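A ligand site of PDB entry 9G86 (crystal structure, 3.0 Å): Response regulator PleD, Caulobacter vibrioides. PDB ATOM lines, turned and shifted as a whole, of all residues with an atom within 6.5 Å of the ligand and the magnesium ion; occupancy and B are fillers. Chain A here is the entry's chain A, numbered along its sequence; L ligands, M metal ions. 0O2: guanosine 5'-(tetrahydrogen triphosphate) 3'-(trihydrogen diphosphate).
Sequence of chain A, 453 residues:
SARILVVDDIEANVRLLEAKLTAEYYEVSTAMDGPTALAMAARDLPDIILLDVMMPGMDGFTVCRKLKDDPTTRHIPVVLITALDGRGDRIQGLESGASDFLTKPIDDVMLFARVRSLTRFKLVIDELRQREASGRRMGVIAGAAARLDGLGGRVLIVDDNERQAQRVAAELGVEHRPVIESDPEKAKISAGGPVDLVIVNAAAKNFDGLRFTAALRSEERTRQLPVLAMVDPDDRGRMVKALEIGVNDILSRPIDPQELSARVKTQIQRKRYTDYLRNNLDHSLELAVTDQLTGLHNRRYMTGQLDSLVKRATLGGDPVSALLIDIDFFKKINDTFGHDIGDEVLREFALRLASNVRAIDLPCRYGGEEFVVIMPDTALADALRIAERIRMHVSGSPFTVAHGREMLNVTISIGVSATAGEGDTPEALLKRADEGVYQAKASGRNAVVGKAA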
ATOM      1  N   LEU A 293      -4.853  19.784  33.807  1.00  0.00           N
ATOM      2  CA  LEU A 293      -4.709  18.497  33.140  1.00  0.00           C
ATOM      3  C   LEU A 293      -3.360  17.866  33.467  1.00  0.00           C
ATOM      4  O   LEU A 293      -3.284  16.820  34.127  1.00  0.00           O
ATOM      5  CB  LEU A 293      -4.903  18.670  31.631  1.00  0.00           C
ATOM      6  CG  LEU A 293      -4.714  17.423  30.778  1.00  0.00           C
ATOM      7  CD1 LEU A 293      -5.923  16.521  30.916  1.00  0.00           C
ATOM      8  CD2 LEU A 293      -4.513  17.808  29.324  1.00  0.00           C
ATOM      9  N   ASP A 326       7.693  20.148  21.293  1.00  0.00           N
ATOM     10  CA  ASP A 326       6.410  20.022  20.609  1.00  0.00           C
ATOM     11  C   ASP A 326       6.182  18.587  20.175  1.00  0.00           C
ATOM     12  O   ASP A 326       7.011  18.016  19.458  1.00  0.00           O
ATOM     13  CB  ASP A 326       6.338  20.959  19.410  1.00  0.00           C
ATOM     14  CG  ASP A 326       4.931  21.178  18.929  1.00  0.00           C
ATOM     15  OD1 ASP A 326       4.143  21.843  19.636  1.00  0.00           O
ATOM     16  OD2 ASP A 326       4.625  20.674  17.833  1.00  0.00           O
ATOM     17  N   ILE A 327       5.067  18.001  20.624  1.00  0.00           N
ATOM     18  CA  ILE A 327       4.711  16.666  20.181  1.00  0.00           C
ATOM     19  C   ILE A 327       4.435  16.694  18.684  1.00  0.00           C
ATOM     20  O   ILE A 327       3.882  17.666  18.159  1.00  0.00           O
ATOM     21  CB  ILE A 327       3.494  16.168  20.980  1.00  0.00           C
ATOM     22  CG1 ILE A 327       3.808  16.220  22.483  1.00  0.00           C
ATOM     23  CG2 ILE A 327       3.102  14.764  20.584  1.00  0.00           C
ATOM     24  CD1 ILE A 327       2.738  15.641  23.367  1.00  0.00           C
ATOM     25  N   ASP A 328       4.825  15.620  17.984  1.00  0.00           N
ATOM     26  CA  ASP A 328       4.701  15.541  16.530  1.00  0.00           C
ATOM     27  C   ASP A 328       3.433  14.774  16.172  1.00  0.00           C
ATOM     28  O   ASP A 328       3.209  13.679  16.690  1.00  0.00           O
ATOM     29  CB  ASP A 328       5.918  14.850  15.918  1.00  0.00           C
ATOM     30  CG  ASP A 328       7.232  15.562  16.228  1.00  0.00           C
ATOM     31  OD1 ASP A 328       7.211  16.803  16.408  1.00  0.00           O
ATOM     32  OD2 ASP A 328       8.281  14.877  16.272  1.00  0.00           O
ATOM     33  N   PHE A 329       2.636  15.351  15.276  1.00  0.00           N
ATOM     34  CA  PHE A 329       1.402  14.730  14.800  1.00  0.00           C
ATOM     35  C   PHE A 329       0.420  14.451  15.936  1.00  0.00           C
ATOM     36  O   PHE A 329      -0.089  13.333  16.082  1.00  0.00           O
ATOM     37  CB  PHE A 329       1.687  13.441  14.021  1.00  0.00           C
ATOM     38  CG  PHE A 329       2.724  13.585  12.953  1.00  0.00           C
ATOM     39  CD1 PHE A 329       2.547  14.499  11.924  1.00  0.00           C
ATOM     40  CD2 PHE A 329       3.853  12.776  12.940  1.00  0.00           C
ATOM     41  CE1 PHE A 329       3.482  14.626  10.922  1.00  0.00           C
ATOM     42  CE2 PHE A 329       4.796  12.902  11.933  1.00  0.00           C
ATOM     43  CZ  PHE A 329       4.613  13.830  10.927  1.00  0.00           C
ATOM     44  N   PHE A 330       0.149  15.477  16.745  1.00  0.00           N
ATOM     45  CA  PHE A 330      -0.842  15.290  17.800  1.00  0.00           C
ATOM     46  C   PHE A 330      -2.249  15.322  17.227  1.00  0.00           C
ATOM     47  O   PHE A 330      -3.150  14.638  17.756  1.00  0.00           O
ATOM     48  CB  PHE A 330      -0.674  16.363  18.882  1.00  0.00           C
ATOM     49  CG  PHE A 330      -1.299  16.000  20.194  1.00  0.00           C
ATOM     50  CD1 PHE A 330      -0.595  15.242  21.129  1.00  0.00           C
ATOM     51  CD2 PHE A 330      -2.584  16.407  20.492  1.00  0.00           C
ATOM     52  CE1 PHE A 330      -1.179  14.900  22.339  1.00  0.00           C
ATOM     53  CE2 PHE A 330      -3.168  16.065  21.702  1.00  0.00           C
ATOM     54  CZ  PHE A 330      -2.464  15.308  22.620  1.00  0.00           C
ATOM     55  N   LYS A 331      -2.459  16.107  16.172  1.00  0.00           N
ATOM     56  CA  LYS A 331      -3.766  16.141  15.515  1.00  0.00           C
ATOM     57  C   LYS A 331      -4.189  14.746  15.073  1.00  0.00           C
ATOM     58  O   LYS A 331      -5.377  14.420  15.125  1.00  0.00           O
ATOM     59  CB  LYS A 331      -3.750  17.106  14.330  1.00  0.00           C
ATOM     60  CG  LYS A 331      -3.737  18.571  14.733  1.00  0.00           C
ATOM     61  CD  LYS A 331      -3.818  19.475  13.508  1.00  0.00           C
ATOM     62  CE  LYS A 331      -3.457  20.909  13.853  1.00  0.00           C
ATOM     63  NZ  LYS A 331      -2.352  21.428  13.012  1.00  0.00           N
ATOM     64  N   LYS A 332      -3.239  13.924  14.609  1.00  0.00           N
ATOM     65  CA  LYS A 332      -3.585  12.554  14.239  1.00  0.00           C
ATOM     66  C   LYS A 332      -4.036  11.759  15.454  1.00  0.00           C
ATOM     67  O   LYS A 332      -4.975  10.950  15.366  1.00  0.00           O
ATOM     68  CB  LYS A 332      -2.393  11.878  13.570  1.00  0.00           C
ATOM     69  CG  LYS A 332      -2.741  10.550  12.891  1.00  0.00           C
ATOM     70  CD  LYS A 332      -3.808  10.723  11.814  1.00  0.00           C
ATOM     71  CE  LYS A 332      -4.099   9.411  11.090  1.00  0.00           C
ATOM     72  NZ  LYS A 332      -2.846   8.747  10.631  1.00  0.00           N
ATOM     73  N   ASN A 334      -5.614  12.968  18.068  1.00  0.00           N
ATOM     74  CA  ASN A 334      -6.984  13.361  18.352  1.00  0.00           C
ATOM     75  C   ASN A 334      -7.956  12.813  17.308  1.00  0.00           C
ATOM     76  O   ASN A 334      -8.965  12.215  17.665  1.00  0.00           O
ATOM     77  CB  ASN A 334      -7.098  14.883  18.420  1.00  0.00           C
ATOM     78  CG  ASN A 334      -6.615  15.450  19.744  1.00  0.00           C
ATOM     79  OD1 ASN A 334      -6.686  14.792  20.778  1.00  0.00           O
ATOM     80  ND2 ASN A 334      -6.087  16.665  19.714  1.00  0.00           N
ATOM     81  N   ASP A 335      -7.566  12.854  16.028  1.00  0.00           N
ATOM     82  CA  ASP A 335      -8.435  12.398  14.957  1.00  0.00           C
ATOM     83  C   ASP A 335      -8.720  10.907  15.085  1.00  0.00           C
ATOM     84  O   ASP A 335      -9.800  10.449  14.698  1.00  0.00           O
ATOM     85  CB  ASP A 335      -7.801  12.684  13.600  1.00  0.00           C
ATOM     86  CG  ASP A 335      -7.808  14.151  13.250  1.00  0.00           C
ATOM     87  OD1 ASP A 335      -8.560  14.908  13.888  1.00  0.00           O
ATOM     88  OD2 ASP A 335      -7.051  14.538  12.336  1.00  0.00           O
ATOM     89  N   GLY A 338      -9.601  10.337  19.787  1.00  0.00           N
ATOM     90  CA  GLY A 338     -10.447  11.230  20.546  1.00  0.00           C
ATOM     91  C   GLY A 338      -9.654  12.169  21.443  1.00  0.00           C
ATOM     92  O   GLY A 338      -8.506  11.906  21.822  1.00  0.00           O
ATOM     93  N   HIS A 339     -10.301  13.263  21.820  1.00  0.00           N
ATOM     94  CA  HIS A 339      -9.636  14.271  22.643  1.00  0.00           C
ATOM     95  C   HIS A 339      -9.325  13.742  24.029  1.00  0.00           C
ATOM     96  O   HIS A 339      -8.345  14.160  24.631  1.00  0.00           O
ATOM     97  CB  HIS A 339     -10.471  15.538  22.720  1.00  0.00           C
ATOM     98  CG  HIS A 339     -10.329  16.411  21.521  1.00  0.00           C
ATOM     99  ND1 HIS A 339     -10.744  16.015  20.267  1.00  0.00           N
ATOM    100  CD2 HIS A 339      -9.808  17.656  21.372  1.00  0.00           C
ATOM    101  CE1 HIS A 339     -10.485  16.976  19.400  1.00  0.00           C
ATOM    102  NE2 HIS A 339      -9.922  17.977  20.041  1.00  0.00           N
ATOM    103  N   ASP A 340     -10.184  12.865  24.564  1.00  0.00           N
ATOM    104  CA  ASP A 340      -9.936  12.328  25.896  1.00  0.00           C
ATOM    105  C   ASP A 340      -8.648  11.511  25.937  1.00  0.00           C
ATOM    106  O   ASP A 340      -7.839  11.641  26.871  1.00  0.00           O
ATOM    107  CB  ASP A 340     -11.149  11.501  26.333  1.00  0.00           C
ATOM    108  CG  ASP A 340     -12.388  12.358  26.550  1.00  0.00           C
ATOM    109  OD1 ASP A 340     -12.266  13.603  26.531  1.00  0.00           O
ATOM    110  OD2 ASP A 340     -13.482  11.785  26.746  1.00  0.00           O
ATOM    111  N   ILE A 341      -8.444  10.667  24.930  1.00  0.00           N
ATOM    112  CA  ILE A 341      -7.192   9.922  24.836  1.00  0.00           C
ATOM    113  C   ILE A 341      -6.026  10.884  24.660  1.00  0.00           C
ATOM    114  O   ILE A 341      -4.948  10.685  25.227  1.00  0.00           O
ATOM    115  CB  ILE A 341      -7.248   8.877  23.718  1.00  0.00           C
ATOM    116  CG1 ILE A 341      -7.925   7.585  24.196  1.00  0.00           C
ATOM    117  CG2 ILE A 341      -5.839   8.548  23.230  1.00  0.00           C
ATOM    118  CD1 ILE A 341      -9.371   7.757  24.655  1.00  0.00           C
ATOM    119  N   GLY A 342      -6.224  11.932  23.841  1.00  0.00           N
ATOM    120  CA  GLY A 342      -5.164  12.931  23.699  1.00  0.00           C
ATOM    121  C   GLY A 342      -4.795  13.581  25.020  1.00  0.00           C
ATOM    122  O   GLY A 342      -3.618  13.793  25.308  1.00  0.00           O
ATOM    123  N   ASP A 343      -5.801  13.887  25.844  1.00  0.00           N
ATOM    124  CA  ASP A 343      -5.558  14.406  27.183  1.00  0.00           C
ATOM    125  C   ASP A 343      -4.762  13.417  28.025  1.00  0.00           C
ATOM    126  O   ASP A 343      -3.855  13.830  28.770  1.00  0.00           O
ATOM    127  CB  ASP A 343      -6.900  14.719  27.856  1.00  0.00           C
ATOM    128  CG  ASP A 343      -7.637  15.874  27.193  1.00  0.00           C
ATOM    129  OD1 ASP A 343      -7.252  16.250  26.062  1.00  0.00           O
ATOM    130  OD2 ASP A 343      -8.625  16.378  27.781  1.00  0.00           O
ATOM    131  N   LEU A 346      -1.183  13.618  26.947  1.00  0.00           N
ATOM    132  CA  LEU A 346      -0.545  14.814  27.486  1.00  0.00           C
ATOM    133  C   LEU A 346      -0.180  14.651  28.959  1.00  0.00           C
ATOM    134  O   LEU A 346       0.921  15.010  29.375  1.00  0.00           O
ATOM    135  CB  LEU A 346      -1.447  16.030  27.280  1.00  0.00           C
ATOM    136  CG  LEU A 346      -1.535  16.554  25.847  1.00  0.00           C
ATOM    137  CD1 LEU A 346      -2.577  17.651  25.741  1.00  0.00           C
ATOM    138  CD2 LEU A 346      -0.171  17.009  25.355  1.00  0.00           C
ATOM    139  N   ARG A 365       3.848  23.768  30.966  1.00  0.00           N
ATOM    140  CA  ARG A 365       3.062  23.633  29.732  1.00  0.00           C
ATOM    141  C   ARG A 365       3.048  24.981  29.021  1.00  0.00           C
ATOM    142  O   ARG A 365       2.330  25.898  29.432  1.00  0.00           O
ATOM    143  CB  ARG A 365       1.661  23.138  30.052  1.00  0.00           C
ATOM    144  CG  ARG A 365       0.952  22.491  28.875  1.00  0.00           C
ATOM    145  CD  ARG A 365      -0.546  22.361  29.135  1.00  0.00           C
ATOM    146  NE  ARG A 365      -1.262  22.019  27.912  1.00  0.00           N
ATOM    147  CZ  ARG A 365      -2.512  21.567  27.863  1.00  0.00           C
ATOM    148  NH1 ARG A 365      -3.214  21.373  28.964  1.00  0.00           N
ATOM    149  NH2 ARG A 365      -3.057  21.287  26.683  1.00  0.00           N
ATOM    150  N   GLY A 367       2.146  25.602  25.725  1.00  0.00           N
ATOM    151  CA  GLY A 367       0.991  25.761  24.859  1.00  0.00           C
ATOM    152  C   GLY A 367       0.026  24.609  25.021  1.00  0.00           C
ATOM    153  O   GLY A 367      -0.051  24.020  26.106  1.00  0.00           O
ATOM    154  N   GLY A 368      -0.697  24.265  23.966  1.00  0.00           N
ATOM    155  CA  GLY A 368      -1.642  23.184  24.093  1.00  0.00           C
ATOM    156  C   GLY A 368      -0.971  21.828  24.042  1.00  0.00           C
ATOM    157  O   GLY A 368      -1.196  20.976  24.905  1.00  0.00           O
ATOM    158  N   GLU A 369      -0.111  21.630  23.042  1.00  0.00           N
ATOM    159  CA  GLU A 369       0.676  20.419  22.886  1.00  0.00           C
ATOM    160  C   GLU A 369       2.156  20.679  23.108  1.00  0.00           C
ATOM    161  O   GLU A 369       2.977  19.767  22.914  1.00  0.00           O
ATOM    162  CB  GLU A 369       0.471  19.803  21.513  1.00  0.00           C
ATOM    163  CG  GLU A 369       1.074  20.624  20.391  1.00  0.00           C
ATOM    164  CD  GLU A 369       1.615  19.760  19.274  1.00  0.00           C
ATOM    165  OE1 GLU A 369       1.488  18.518  19.374  1.00  0.00           O
ATOM    166  OE2 GLU A 369       2.111  20.310  18.288  1.00  0.00           O
ATOM    167  N   SER A 413       9.662  17.025  18.743  1.00  0.00           N
ATOM    168  CA  SER A 413      10.697  17.896  18.200  1.00  0.00           C
ATOM    169  C   SER A 413      11.062  18.930  19.255  1.00  0.00           C
ATOM    170  O   SER A 413      10.173  19.555  19.841  1.00  0.00           O
ATOM    171  CB  SER A 413      10.233  18.579  16.918  1.00  0.00           C
ATOM    172  OG  SER A 413       9.837  17.638  15.944  1.00  0.00           O
ATOM    173  N   LYS A 441      11.047  20.660  13.008  1.00  0.00           N
ATOM    174  CA  LYS A 441       9.846  20.176  12.327  1.00  0.00           C
ATOM    175  C   LYS A 441      10.063  20.102  10.817  1.00  0.00           C
ATOM    176  O   LYS A 441       9.532  19.198  10.154  1.00  0.00           O
ATOM    177  CB  LYS A 441       8.648  21.068  12.668  1.00  0.00           C
ATOM    178  N   ARG A 445      11.349  14.910  11.678  1.00  0.00           N
ATOM    179  CA  ARG A 445      10.898  15.160  13.049  1.00  0.00           C
ATOM    180  C   ARG A 445      11.779  14.317  13.971  1.00  0.00           C
ATOM    181  O   ARG A 445      12.828  13.827  13.559  1.00  0.00           O
ATOM    182  CB  ARG A 445       9.388  14.918  13.186  1.00  0.00           C
ATOM    183  CG  ARG A 445       8.558  15.983  12.476  1.00  0.00           C
ATOM    184  CD  ARG A 445       7.072  15.706  12.530  1.00  0.00           C
ATOM    185  NE  ARG A 445       6.316  16.896  12.153  1.00  0.00           N
ATOM    186  CZ  ARG A 445       6.126  17.310  10.907  1.00  0.00           C
ATOM    187  NH1 ARG A 445       6.572  16.607   9.873  1.00  0.00           N
ATOM    188  NH2 ARG A 445       5.462  18.438  10.690  1.00  0.00           N
HETATM  189  PD  0O2 L   1      -7.822  19.328  17.705  1.00  0.00           P
HETATM  190  O1D 0O2 L   1      -6.934  18.900  18.849  1.00  0.00           O
HETATM  191  O2D 0O2 L   1      -7.425  18.583  16.447  1.00  0.00           O
HETATM  192  O3D 0O2 L   1      -9.276  19.115  18.024  1.00  0.00           O
HETATM  193  PG  0O2 L   1       3.246  18.880  14.227  1.00  0.00           P
HETATM  194  O1G 0O2 L   1       2.740  20.128  13.546  1.00  0.00           O
HETATM  195  O2G 0O2 L   1       3.722  17.901  13.177  1.00  0.00           O
HETATM  196  O3G 0O2 L   1       4.376  19.245  15.159  1.00  0.00           O
HETATM  197  PB  0O2 L   1       0.586  18.863  15.348  1.00  0.00           P
HETATM  198  O1B 0O2 L   1      -0.119  18.152  16.464  1.00  0.00           O
HETATM  199  O2B 0O2 L   1      -0.254  18.795  14.094  1.00  0.00           O
HETATM  200  O3B 0O2 L   1       2.037  18.154  15.094  1.00  0.00           O
HETATM  201  O3A 0O2 L   1       0.886  20.457  15.702  1.00  0.00           O
HETATM  202  PA  0O2 L   1      -0.078  21.494  16.531  1.00  0.00           P
HETATM  203  O1A 0O2 L   1      -1.113  22.104  15.620  1.00  0.00           O
HETATM  204  O2A 0O2 L   1       0.814  22.576  17.086  1.00  0.00           O
HETATM  205  O5' 0O2 L   1      -0.832  20.698  17.768  1.00  0.00           O
HETATM  206  C5' 0O2 L   1      -1.840  21.338  18.531  1.00  0.00           C
HETATM  207  C4' 0O2 L   1      -2.895  20.445  18.679  1.00  0.00           C
HETATM  208  O4' 0O2 L   1      -2.973  19.844  20.064  1.00  0.00           O
HETATM  209  C3' 0O2 L   1      -4.275  21.222  18.494  1.00  0.00           C
HETATM  210  O3' 0O2 L   1      -5.072  20.509  17.449  1.00  0.00           O
HETATM  211  C2' 0O2 L   1      -4.831  21.219  19.616  1.00  0.00           C
HETATM  212  O2' 0O2 L   1      -6.307  21.079  19.645  1.00  0.00           O
HETATM  213  C1' 0O2 L   1      -4.220  19.937  20.453  1.00  0.00           C
HETATM  214  N9  0O2 L   1      -4.308  20.352  21.807  1.00  0.00           N
HETATM  215  C8  0O2 L   1      -3.920  21.404  22.540  1.00  0.00           C
HETATM  216  N7  0O2 L   1      -4.348  21.205  23.809  1.00  0.00           N
HETATM  217  C5  0O2 L   1      -4.992  20.038  23.839  1.00  0.00           C
HETATM  218  C6  0O2 L   1      -5.670  19.292  24.982  1.00  0.00           C
HETATM  219  O6  0O2 L   1      -5.687  19.748  26.080  1.00  0.00           O
HETATM  220  N1  0O2 L   1      -6.300  18.040  24.729  1.00  0.00           N
HETATM  221  C2  0O2 L   1      -6.275  17.491  23.394  1.00  0.00           C
HETATM  222  N2  0O2 L   1      -6.904  16.220  23.111  1.00  0.00           N
HETATM  223  N3  0O2 L   1      -5.624  18.202  22.306  1.00  0.00           N
HETATM  224  C4  0O2 L   1      -4.973  19.513  22.580  1.00  0.00           C
HETATM  225  PC  0O2 L   1      -6.243  21.413  16.768  1.00  0.00           P
HETATM  226  O1C 0O2 L   1      -5.976  22.856  17.099  1.00  0.00           O
HETATM  227  O2C 0O2 L   1      -6.318  21.127  15.279  1.00  0.00           O
HETATM  228  O3C 0O2 L   1      -7.634  20.928  17.471  1.00  0.00           O
HETATM  229 MG    MG M   1       2.940  19.226  16.973  1.00  0.00          MG
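O of Asp 326 sits at hydrogen-bond distance from N of Ser 413. The guanidinium group of Arg 365 sits at hydrogen-bond distance from the backbone carbonyl oxygen of Gly 368 (2.6 Å). The guanidinium group (NE) of Arg 365 sits at hydrogen-bond distance from the backbone carbonyl oxygen (O) of Gly 367, 3.0 Å away. OD1 of Asp 328 sits at hydrogen-bond distance from OG of Ser 413 (2.8 Å).
A nitrogen (N7) of the ligand lies close to the backbone carbonyl oxygen of Gly 368. Leu 293 touches the ligand. C of Asp 328 touches O3B of the ligand (3.8 Å). Gly 342 touches the ligand (CA to N2, 3.8 Å). Leu 346 touches the ligand (CD1 to C6, 3.6 Å). Hydrophobic or aromatic side chains within 4 Å of the ligand: Leu 293, Phe 329, Phe 330, His 339 and Leu 346. Of the 24 residues printed, 16 come within 4 Å of the ligand. The nearest printed residue that does not touch the ligand is Asp 335 (4.6 Å).
Three residues have an atom within 4 Å of the magnesium ion: Asp 326, Ile 327 and Glu 369. The nearest printed residue that does not touch the magnesium ion is Asp 328 (4.1 Å).
The magnesium ion is bound by OE2 of Glu 369, O of Ile 327, O3G of the ligand, O3B of the ligand and OD2 of Asp 326. The magnesium ion has five donor atoms within binding distance. Slightly farther from the magnesium ion lies an oxygen (O3A) of the ligand (2.7 Å).
A nitrogen (N2) of the ligand is in hydrogen-bond range of the backbone carbonyl oxygen of His 339. An oxygen (O3D) of the ligand lies within hydrogen-bond range of a ring nitrogen (NE2) of His 339, at 2.4 Å. A nitrogen (N1) of the ligand is in hydrogen-bond range of the side-chain carboxylate (OD1) of Asp 343 (2.4 Å). The side-chain amide nitrogen of Asn 334 sits at hydrogen-bond distance from an oxygen (O1D) of the ligand (2.5 Å). The backbone NH (N) of Phe 330 lies within hydrogen-bond range of an oxygen (O1B) of the ligand, at 2.7 Å. An oxygen (O2G) of the ligand sits at hydrogen-bond distance from the backbone NH (N) of Phe 329 (3.5 Å). O2G of the ligand lies within salt-bridge range of NE of Arg 445, at 3.0 Å. The backbone NH (N) of Lys 331 sits at hydrogen-bond distance from an oxygen (O1B) of the ligand (3.1 Å). NZ of Lys 331 lies within salt-bridge range of O1A of the ligand, at 3.0 Å. The guanidinium group (NH2) of Arg 365 is in hydrogen-bond range of an oxygen (O6) of the ligand (3.1 Å).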
